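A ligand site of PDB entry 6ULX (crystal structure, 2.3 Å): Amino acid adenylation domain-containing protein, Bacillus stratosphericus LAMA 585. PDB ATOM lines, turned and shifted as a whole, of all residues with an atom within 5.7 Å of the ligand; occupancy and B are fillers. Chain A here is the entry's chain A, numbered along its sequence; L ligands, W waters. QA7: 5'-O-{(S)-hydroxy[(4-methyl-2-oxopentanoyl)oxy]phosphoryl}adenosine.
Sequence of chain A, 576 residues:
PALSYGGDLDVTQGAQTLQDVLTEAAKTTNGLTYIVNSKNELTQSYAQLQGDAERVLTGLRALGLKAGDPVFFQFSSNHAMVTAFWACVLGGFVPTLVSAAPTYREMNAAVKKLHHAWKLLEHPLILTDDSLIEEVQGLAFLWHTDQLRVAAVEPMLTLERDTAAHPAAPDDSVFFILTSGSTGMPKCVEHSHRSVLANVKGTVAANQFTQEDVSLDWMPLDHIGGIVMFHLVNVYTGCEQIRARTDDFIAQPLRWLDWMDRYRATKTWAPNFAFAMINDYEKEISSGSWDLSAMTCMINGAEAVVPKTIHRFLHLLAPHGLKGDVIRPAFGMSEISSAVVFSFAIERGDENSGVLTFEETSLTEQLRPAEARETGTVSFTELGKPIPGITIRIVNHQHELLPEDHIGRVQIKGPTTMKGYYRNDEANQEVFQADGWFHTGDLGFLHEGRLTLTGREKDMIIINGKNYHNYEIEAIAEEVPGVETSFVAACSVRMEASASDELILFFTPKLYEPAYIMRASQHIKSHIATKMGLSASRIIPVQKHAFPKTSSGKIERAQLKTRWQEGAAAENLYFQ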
ATOM      1  N   THR A 179      25.243 -31.040  19.639  1.00  0.00           N
ATOM      2  CA  THR A 179      25.502 -29.627  19.442  1.00  0.00           C
ATOM      3  C   THR A 179      24.608 -29.091  18.328  1.00  0.00           C
ATOM      4  O   THR A 179      23.742 -29.787  17.795  1.00  0.00           O
ATOM      5  CB  THR A 179      26.977 -29.404  19.104  1.00  0.00           C
ATOM      6  OG1 THR A 179      27.280 -30.012  17.839  1.00  0.00           O
ATOM      7  CG2 THR A 179      27.876 -30.003  20.170  1.00  0.00           C
ATOM      8  N   SER A 180      24.830 -27.823  17.962  1.00  0.00           N
ATOM      9  CA  SER A 180      24.139 -27.225  16.830  1.00  0.00           C
ATOM     10  C   SER A 180      24.934 -27.343  15.545  1.00  0.00           C
ATOM     11  O   SER A 180      24.345 -27.457  14.454  1.00  0.00           O
ATOM     12  CB  SER A 180      23.848 -25.745  17.108  1.00  0.00           C
ATOM     13  OG  SER A 180      24.749 -24.907  16.395  1.00  0.00           O
ATOM     14  N   HIS A 223      18.911 -28.892  25.943  1.00  0.00           N
ATOM     15  CA  HIS A 223      19.903 -27.823  25.970  1.00  0.00           C
ATOM     16  C   HIS A 223      20.755 -27.971  27.215  1.00  0.00           C
ATOM     17  O   HIS A 223      20.238 -28.248  28.309  1.00  0.00           O
ATOM     18  CB  HIS A 223      19.209 -26.449  25.964  1.00  0.00           C
ATOM     19  CG  HIS A 223      20.132 -25.314  25.673  1.00  0.00           C
ATOM     20  ND1 HIS A 223      21.125 -24.925  26.551  1.00  0.00           N
ATOM     21  CD2 HIS A 223      20.209 -24.467  24.622  1.00  0.00           C
ATOM     22  CE1 HIS A 223      21.772 -23.894  26.041  1.00  0.00           C
ATOM     23  NE2 HIS A 223      21.230 -23.594  24.869  1.00  0.00           N
ATOM     24  N   ILE A 224      22.064 -27.798  27.060  1.00  0.00           N
ATOM     25  CA  ILE A 224      22.990 -28.067  28.158  1.00  0.00           C
ATOM     26  C   ILE A 224      22.640 -27.216  29.378  1.00  0.00           C
ATOM     27  O   ILE A 224      22.770 -27.665  30.520  1.00  0.00           O
ATOM     28  CB  ILE A 224      24.445 -27.836  27.700  1.00  0.00           C
ATOM     29  CG1 ILE A 224      25.426 -28.426  28.727  1.00  0.00           C
ATOM     30  CG2 ILE A 224      24.714 -26.353  27.504  1.00  0.00           C
ATOM     31  CD1 ILE A 224      25.462 -29.946  28.732  1.00  0.00           C
ATOM     32  N   GLY A 225      22.199 -25.970  29.152  1.00  0.00           N
ATOM     33  CA  GLY A 225      21.792 -25.117  30.249  1.00  0.00           C
ATOM     34  C   GLY A 225      20.510 -25.561  30.925  1.00  0.00           C
ATOM     35  O   GLY A 225      20.290 -25.229  32.089  1.00  0.00           O
ATOM     36  N   MET A 229      22.951 -26.736  33.974  1.00  0.00           N
ATOM     37  CA  MET A 229      23.001 -25.482  34.724  1.00  0.00           C
ATOM     38  C   MET A 229      21.827 -25.332  35.690  1.00  0.00           C
ATOM     39  O   MET A 229      21.973 -24.737  36.762  1.00  0.00           O
ATOM     40  CB  MET A 229      23.023 -24.288  33.764  1.00  0.00           C
ATOM     41  CG  MET A 229      23.147 -22.950  34.464  1.00  0.00           C
ATOM     42  SD  MET A 229      23.400 -21.561  33.334  1.00  0.00           S
ATOM     43  CE  MET A 229      21.815 -21.507  32.501  1.00  0.00           C
ATOM     44  N   TRP A 269      16.255 -18.502  33.895  1.00  0.00           N
ATOM     45  CA  TRP A 269      17.224 -18.141  32.871  1.00  0.00           C
ATOM     46  C   TRP A 269      16.567 -18.237  31.497  1.00  0.00           C
ATOM     47  O   TRP A 269      15.467 -18.780  31.340  1.00  0.00           O
ATOM     48  CB  TRP A 269      18.466 -19.046  32.923  1.00  0.00           C
ATOM     49  CG  TRP A 269      18.319 -20.342  32.188  1.00  0.00           C
ATOM     50  CD1 TRP A 269      17.627 -21.448  32.594  1.00  0.00           C
ATOM     51  CD2 TRP A 269      18.891 -20.684  30.922  1.00  0.00           C
ATOM     52  NE1 TRP A 269      17.734 -22.443  31.655  1.00  0.00           N
ATOM     53  CE2 TRP A 269      18.501 -22.002  30.616  1.00  0.00           C
ATOM     54  CE3 TRP A 269      19.706 -19.986  30.002  1.00  0.00           C
ATOM     55  CZ2 TRP A 269      18.899 -22.641  29.440  1.00  0.00           C
ATOM     56  CZ3 TRP A 269      20.093 -20.628  28.845  1.00  0.00           C
ATOM     57  CH2 TRP A 269      19.690 -21.942  28.574  1.00  0.00           C
ATOM     58  N   ILE A 299      19.511 -15.496  34.833  1.00  0.00           N
ATOM     59  CA  ILE A 299      20.703 -15.747  34.034  1.00  0.00           C
ATOM     60  C   ILE A 299      20.370 -15.532  32.561  1.00  0.00           C
ATOM     61  O   ILE A 299      19.342 -16.002  32.080  1.00  0.00           O
ATOM     62  CB  ILE A 299      21.244 -17.165  34.279  1.00  0.00           C
ATOM     63  CG1 ILE A 299      21.874 -17.246  35.680  1.00  0.00           C
ATOM     64  CG2 ILE A 299      22.230 -17.567  33.201  1.00  0.00           C
ATOM     65  CD1 ILE A 299      22.121 -18.661  36.170  1.00  0.00           C
ATOM     66  N   ASN A 300      21.257 -14.818  31.859  1.00  0.00           N
ATOM     67  CA  ASN A 300      21.101 -14.532  30.437  1.00  0.00           C
ATOM     68  C   ASN A 300      22.324 -15.091  29.712  1.00  0.00           C
ATOM     69  O   ASN A 300      23.437 -14.584  29.887  1.00  0.00           O
ATOM     70  CB  ASN A 300      20.953 -13.028  30.191  1.00  0.00           C
ATOM     71  CG  ASN A 300      20.725 -12.685  28.735  1.00  0.00           C
ATOM     72  OD1 ASN A 300      21.058 -13.458  27.836  1.00  0.00           O
ATOM     73  ND2 ASN A 300      20.167 -11.513  28.492  1.00  0.00           N
ATOM     74  N   GLY A 301      22.129 -16.130  28.913  1.00  0.00           N
ATOM     75  CA  GLY A 301      23.242 -16.745  28.220  1.00  0.00           C
ATOM     76  C   GLY A 301      22.756 -17.665  27.130  1.00  0.00           C
ATOM     77  O   GLY A 301      21.558 -17.957  27.014  1.00  0.00           O
ATOM     78  N   ALA A 302      23.724 -18.135  26.330  1.00  0.00           N
ATOM     79  CA  ALA A 302      23.541 -19.031  25.193  1.00  0.00           C
ATOM     80  C   ALA A 302      23.704 -18.263  23.887  1.00  0.00           C
ATOM     81  O   ALA A 302      23.889 -18.870  22.826  1.00  0.00           O
ATOM     82  CB  ALA A 302      22.185 -19.727  25.223  1.00  0.00           C
ATOM     83  N   GLU A 303      23.645 -16.940  23.950  1.00  0.00           N
ATOM     84  CA  GLU A 303      23.831 -16.100  22.774  1.00  0.00           C
ATOM     85  C   GLU A 303      24.238 -14.707  23.252  1.00  0.00           C
ATOM     86  O   GLU A 303      24.321 -14.442  24.454  1.00  0.00           O
ATOM     87  CB  GLU A 303      22.580 -16.057  21.901  1.00  0.00           C
ATOM     88  CG  GLU A 303      21.385 -15.371  22.546  1.00  0.00           C
ATOM     89  CD  GLU A 303      20.140 -15.488  21.696  1.00  0.00           C
ATOM     90  OE1 GLU A 303      20.056 -16.411  20.869  1.00  0.00           O
ATOM     91  OE2 GLU A 303      19.228 -14.647  21.850  1.00  0.00           O
ATOM     92  N   ALA A 304      24.508 -13.822  22.294  1.00  0.00           N
ATOM     93  CA  ALA A 304      25.019 -12.502  22.619  1.00  0.00           C
ATOM     94  C   ALA A 304      24.062 -11.773  23.552  1.00  0.00           C
ATOM     95  O   ALA A 304      22.870 -11.637  23.262  1.00  0.00           O
ATOM     96  CB  ALA A 304      25.242 -11.694  21.335  1.00  0.00           C
ATOM     97  N   VAL A 305      24.601 -11.298  24.671  1.00  0.00           N
ATOM     98  CA  VAL A 305      23.825 -10.528  25.644  1.00  0.00           C
ATOM     99  C   VAL A 305      23.895  -9.061  25.254  1.00  0.00           C
ATOM    100  O   VAL A 305      24.975  -8.461  25.255  1.00  0.00           O
ATOM    101  CB  VAL A 305      24.355 -10.747  27.070  1.00  0.00           C
ATOM    102  CG1 VAL A 305      23.491  -9.993  28.072  1.00  0.00           C
ATOM    103  CG2 VAL A 305      24.389 -12.234  27.398  1.00  0.00           C
ATOM    104  N   ALA A 330      25.950 -14.782  31.283  1.00  0.00           N
ATOM    105  CA  ALA A 330      26.764 -15.983  31.421  1.00  0.00           C
ATOM    106  C   ALA A 330      27.129 -16.521  30.037  1.00  0.00           C
ATOM    107  O   ALA A 330      26.445 -16.254  29.049  1.00  0.00           O
ATOM    108  CB  ALA A 330      26.032 -17.066  32.220  1.00  0.00           C
ATOM    109  N   PHE A 331      28.232 -17.274  29.992  1.00  0.00           N
ATOM    110  CA  PHE A 331      28.682 -17.943  28.784  1.00  0.00           C
ATOM    111  C   PHE A 331      29.030 -19.384  29.101  1.00  0.00           C
ATOM    112  O   PHE A 331      29.536 -19.700  30.180  1.00  0.00           O
ATOM    113  CB  PHE A 331      29.896 -17.235  28.159  1.00  0.00           C
ATOM    114  CG  PHE A 331      30.804 -18.160  27.399  1.00  0.00           C
ATOM    115  CD1 PHE A 331      30.498 -18.554  26.110  1.00  0.00           C
ATOM    116  CD2 PHE A 331      31.967 -18.634  27.979  1.00  0.00           C
ATOM    117  CE1 PHE A 331      31.335 -19.401  25.408  1.00  0.00           C
ATOM    118  CE2 PHE A 331      32.808 -19.493  27.284  1.00  0.00           C
ATOM    119  CZ  PHE A 331      32.490 -19.875  25.995  1.00  0.00           C
ATOM    120  N   GLY A 332      28.765 -20.268  28.146  1.00  0.00           N
ATOM    121  CA  GLY A 332      29.131 -21.663  28.291  1.00  0.00           C
ATOM    122  C   GLY A 332      28.935 -22.395  26.976  1.00  0.00           C
ATOM    123  O   GLY A 332      28.514 -21.818  25.980  1.00  0.00           O
ATOM    124  N   MET A 333      29.250 -23.688  27.012  1.00  0.00           N
ATOM    125  CA  MET A 333      29.095 -24.539  25.845  1.00  0.00           C
ATOM    126  C   MET A 333      28.691 -25.937  26.293  1.00  0.00           C
ATOM    127  O   MET A 333      28.924 -26.329  27.446  1.00  0.00           O
ATOM    128  CB  MET A 333      30.382 -24.609  25.013  1.00  0.00           C
ATOM    129  CG  MET A 333      31.013 -23.269  24.705  1.00  0.00           C
ATOM    130  SD  MET A 333      32.635 -23.453  23.925  1.00  0.00           S
ATOM    131  CE  MET A 333      32.202 -24.332  22.427  1.00  0.00           C
ATOM    132  N   SER A 334      28.090 -26.686  25.381  1.00  0.00           N
ATOM    133  CA  SER A 334      27.806 -28.090  25.648  1.00  0.00           C
ATOM    134  C   SER A 334      29.093 -28.853  25.972  1.00  0.00           C
ATOM    135  O   SER A 334      29.104 -29.714  26.848  1.00  0.00           O
ATOM    136  CB  SER A 334      27.108 -28.734  24.448  1.00  0.00           C
ATOM    137  OG  SER A 334      25.838 -28.141  24.234  1.00  0.00           O
ATOM    138  N   GLU A 335      30.187 -28.534  25.261  1.00  0.00           N
ATOM    139  CA  GLU A 335      31.425 -29.270  25.440  1.00  0.00           C
ATOM    140  C   GLU A 335      32.013 -29.120  26.840  1.00  0.00           C
ATOM    141  O   GLU A 335      32.793 -29.977  27.264  1.00  0.00           O
ATOM    142  CB  GLU A 335      32.454 -28.830  24.400  1.00  0.00           C
ATOM    143  CG  GLU A 335      32.127 -29.243  22.970  1.00  0.00           C
ATOM    144  CD  GLU A 335      31.135 -28.317  22.299  1.00  0.00           C
ATOM    145  OE1 GLU A 335      30.570 -27.427  22.980  1.00  0.00           O
ATOM    146  OE2 GLU A 335      30.916 -28.458  21.077  1.00  0.00           O
ATOM    147  N   SER A 338      27.966 -26.594  30.066  1.00  0.00           N
ATOM    148  CA  SER A 338      27.200 -25.378  30.309  1.00  0.00           C
ATOM    149  C   SER A 338      28.082 -24.248  30.825  1.00  0.00           C
ATOM    150  O   SER A 338      29.272 -24.190  30.504  1.00  0.00           O
ATOM    151  CB  SER A 338      26.049 -25.648  31.296  1.00  0.00           C
ATOM    152  OG  SER A 338      26.490 -25.603  32.651  1.00  0.00           O
ATOM    153  N   ALA A 339      27.506 -23.349  31.615  1.00  0.00           N
ATOM    154  CA  ALA A 339      28.154 -22.070  31.910  1.00  0.00           C
ATOM    155  C   ALA A 339      29.459 -22.262  32.678  1.00  0.00           C
ATOM    156  O   ALA A 339      29.581 -23.150  33.521  1.00  0.00           O
ATOM    157  CB  ALA A 339      27.204 -21.170  32.715  1.00  0.00           C
ATOM    158  N   LEU A 383      30.815 -10.906  30.820  1.00  0.00           N
ATOM    159  CA  LEU A 383      30.218 -12.183  31.199  1.00  0.00           C
ATOM    160  C   LEU A 383      30.807 -12.740  32.486  1.00  0.00           C
ATOM    161  O   LEU A 383      30.376 -13.813  32.924  1.00  0.00           O
ATOM    162  CB  LEU A 383      30.396 -13.194  30.059  1.00  0.00           C
ATOM    163  CG  LEU A 383      29.876 -12.684  28.712  1.00  0.00           C
ATOM    164  CD1 LEU A 383      30.049 -13.725  27.616  1.00  0.00           C
ATOM    165  CD2 LEU A 383      28.411 -12.260  28.814  1.00  0.00           C
ATOM    166  N   THR A 440      37.509 -23.112  22.129  1.00  0.00           N
ATOM    167  CA  THR A 440      36.066 -22.880  22.060  1.00  0.00           C
ATOM    168  C   THR A 440      35.604 -22.538  20.649  1.00  0.00           C
ATOM    169  O   THR A 440      34.489 -22.895  20.259  1.00  0.00           O
ATOM    170  CB  THR A 440      35.665 -21.749  23.013  1.00  0.00           C
ATOM    171  OG1 THR A 440      36.262 -20.518  22.559  1.00  0.00           O
ATOM    172  CG2 THR A 440      36.119 -22.050  24.430  1.00  0.00           C
ATOM    173  N   ASP A 442      35.279 -19.386  19.935  1.00  0.00           N
ATOM    174  CA  ASP A 442      34.740 -18.051  20.161  1.00  0.00           C
ATOM    175  C   ASP A 442      35.874 -17.039  20.275  1.00  0.00           C
ATOM    176  O   ASP A 442      37.035 -17.377  20.513  1.00  0.00           O
ATOM    177  CB  ASP A 442      33.896 -18.019  21.442  1.00  0.00           C
ATOM    178  CG  ASP A 442      32.677 -18.911  21.347  1.00  0.00           C
ATOM    179  OD1 ASP A 442      31.924 -18.801  20.359  1.00  0.00           O
ATOM    180  OD2 ASP A 442      32.482 -19.744  22.258  1.00  0.00           O
ATOM    181  N   LEU A 453      32.889 -11.761  25.322  1.00  0.00           N
ATOM    182  CA  LEU A 453      32.902 -12.293  23.965  1.00  0.00           C
ATOM    183  C   LEU A 453      32.582 -11.190  22.958  1.00  0.00           C
ATOM    184  O   LEU A 453      31.774 -10.296  23.233  1.00  0.00           O
ATOM    185  CB  LEU A 453      31.911 -13.440  23.827  1.00  0.00           C
ATOM    186  CG  LEU A 453      32.242 -14.741  24.556  1.00  0.00           C
ATOM    187  CD1 LEU A 453      31.224 -15.817  24.198  1.00  0.00           C
ATOM    188  CD2 LEU A 453      33.648 -15.218  24.254  1.00  0.00           C
ATOM    189  N   ARG A 456      33.033 -14.828  16.712  1.00  0.00           N
ATOM    190  CA  ARG A 456      33.358 -16.228  16.523  1.00  0.00           C
ATOM    191  C   ARG A 456      34.283 -16.380  15.325  1.00  0.00           C
ATOM    192  O   ARG A 456      34.176 -15.631  14.356  1.00  0.00           O
ATOM    193  CB  ARG A 456      32.098 -17.073  16.333  1.00  0.00           C
ATOM    194  CG  ARG A 456      30.950 -16.721  17.255  1.00  0.00           C
ATOM    195  CD  ARG A 456      29.781 -17.680  17.107  1.00  0.00           C
ATOM    196  NE  ARG A 456      29.328 -17.796  15.714  1.00  0.00           N
ATOM    197  CZ  ARG A 456      28.499 -16.939  15.124  1.00  0.00           C
ATOM    198  NH1 ARG A 456      28.028 -15.892  15.788  1.00  0.00           N
ATOM    199  NH2 ARG A 456      28.142 -17.125  13.856  1.00  0.00           N
HETATM  200  C01 QA7 L   1      24.408 -22.473  29.412  1.00  0.00           C
HETATM  201  C02 QA7 L   1      25.303 -21.394  28.825  1.00  0.00           C
HETATM  202  C03 QA7 L   1      24.929 -20.054  29.463  1.00  0.00           C
HETATM  203  C04 QA7 L   1      25.245 -21.377  27.307  1.00  0.00           C
HETATM  204  C05 QA7 L   1      25.609 -22.734  26.708  1.00  0.00           C
HETATM  205  C06 QA7 L   1      25.316 -23.030  25.242  1.00  0.00           C
HETATM  206  C10 QA7 L   1      27.738 -22.652  22.754  1.00  0.00           C
HETATM  207  C11 QA7 L   1      27.968 -21.500  22.015  1.00  0.00           C
HETATM  208  C12 QA7 L   1      29.348 -20.788  22.419  1.00  0.00           C
HETATM  209  C13 QA7 L   1      29.209 -19.623  22.066  1.00  0.00           C
HETATM  210  C14 QA7 L   1      27.579 -19.284  22.279  1.00  0.00           C
HETATM  211  C16 QA7 L   1      27.015 -19.034  24.677  1.00  0.00           C
HETATM  212  C18 QA7 L   1      27.182 -16.865  24.891  1.00  0.00           C
HETATM  213  C19 QA7 L   1      27.220 -15.487  25.264  1.00  0.00           C
HETATM  214  C21 QA7 L   1      27.819 -14.928  23.108  1.00  0.00           C
HETATM  215  C23 QA7 L   1      27.473 -17.177  23.599  1.00  0.00           C
HETATM  216  N15 QA7 L   1      27.363 -18.529  23.480  1.00  0.00           N
HETATM  217  N17 QA7 L   1      26.902 -18.015  25.553  1.00  0.00           N
HETATM  218  N20 QA7 L   1      27.542 -14.570  24.368  1.00  0.00           N
HETATM  219  N22 QA7 L   1      27.789 -16.189  22.715  1.00  0.00           N
HETATM  220  N24 QA7 L   1      26.935 -15.108  26.621  1.00  0.00           N
HETATM  221  O07 QA7 L   1      25.564 -24.307  24.670  1.00  0.00           O
HETATM  222  O09 QA7 L   1      26.569 -23.254  22.291  1.00  0.00           O
HETATM  223  O25 QA7 L   1      26.957 -20.405  22.336  1.00  0.00           O
HETATM  224  O26 QA7 L   1      29.513 -19.390  20.631  1.00  0.00           O
HETATM  225  O27 QA7 L   1      30.502 -21.494  21.747  1.00  0.00           O
HETATM  226  O28 QA7 L   1      26.994 -25.676  22.908  1.00  0.00           O
HETATM  227  O29 QA7 L   1      24.690 -25.026  22.350  1.00  0.00           O
HETATM  228  O30 QA7 L   1      24.871 -22.129  24.618  1.00  0.00           O
HETATM  229  O31 QA7 L   1      26.105 -23.562  27.393  1.00  0.00           O
HETATM  230  P08 QA7 L   1      25.956 -24.583  23.061  1.00  0.00           P
HETATM  231  O   HOH W   1      28.815 -25.883  21.268  1.00  0.00           O
HETATM  232  O   HOH W   2      31.903 -20.553  18.424  1.00  0.00           O
HETATM  233  O   HOH W   3      27.477 -11.870  25.118  1.00  0.00           O
HETATM  234  O   HOH W   4      23.141 -27.178  24.306  1.00  0.00           O
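An oxygen (O28) of the ligand sits at hydrogen-bond distance from the side-chain hydroxyl (OG) of Ser 334 (3.0 Å).
O28 of the ligand sits at hydrogen-bond distance from N of Ser 334.
N24 of the ligand sits at hydrogen-bond distance from O of Ala 330, 2.7 Å away.
The side-chain sulfur of Met 333 sits close to an oxygen (O27) of the ligand, 3.6 Å away.
An oxygen (O31) of the ligand lies within hydrogen-bond range of the backbone NH (N) of Met 333 (3.2 Å).
The backbone carbonyl oxygen (O) of Glu 303 sits close to a nitrogen (N24) of the ligand (3.5 Å).
A nitrogen (N17) of the ligand sits at hydrogen-bond distance from the backbone NH (N) of Ala 302 (3.3 Å).
O26 of the ligand is in hydrogen-bond range of OD1 of Asp 442 (2.5 Å).
O of Asn 300 sits at hydrogen-bond distance from N of Ala 330, 2.9 Å away.
N of Gly 225 is in hydrogen-bond range of ND1 of His 223 (3.0 Å).
The backbone carbonyl oxygen (O) of Met 333 is in hydrogen-bond range of the backbone NH (N) of Ser 338, at 2.8 Å.
The backbone NH of Asp 442 lies within hydrogen-bond range of the side-chain hydroxyl of Thr 440, 3.0 Å away.
The backbone carbonyl oxygen (O) of Gly 332 lies close to an oxygen (O31) of the ligand.
Merely in contact with the ligand: Ile 224 (3.1 Å), Leu 383 (3.5 Å), Ala 304 (3.6 Å), Ser 338 (3.6 Å), Phe 331 (3.7 Å), Leu 453 (3.7 Å), His 223 (3.7 Å), Gly 225 (3.8 Å), Ala 339 (3.9 Å), Gly 301 (3.9 Å), Val 305 (3.9 Å), Arg 456 (3.9 Å) and Glu 335 (3.98 Å).
Hydrophobic or aromatic side chains that line the ligand: His 223, Ile 224, Ala 302, Val 305, Phe 331, Met 333, Leu 383 and Leu 453.
Along chain A the residues within 4 Å of the ligand span positions 223 to 456.
Water W1 lies within hydrogen-bond range of O28 of the ligand and OE1 of Glu 335.
Water W3 bridges N20 of the ligand (2.8 Å) and N of Val 305 (3.0 Å).
Water W4 lies within hydrogen-bond range of OG of Ser 334 (2.9 Å), N of Ile 224 (3.0 Å) and O29 of the ligand (3.3 Å).
Water W2 lies within hydrogen-bond range of the side-chain carboxylate (OD1) of Asp 442 and an oxygen (O26) of the ligand.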
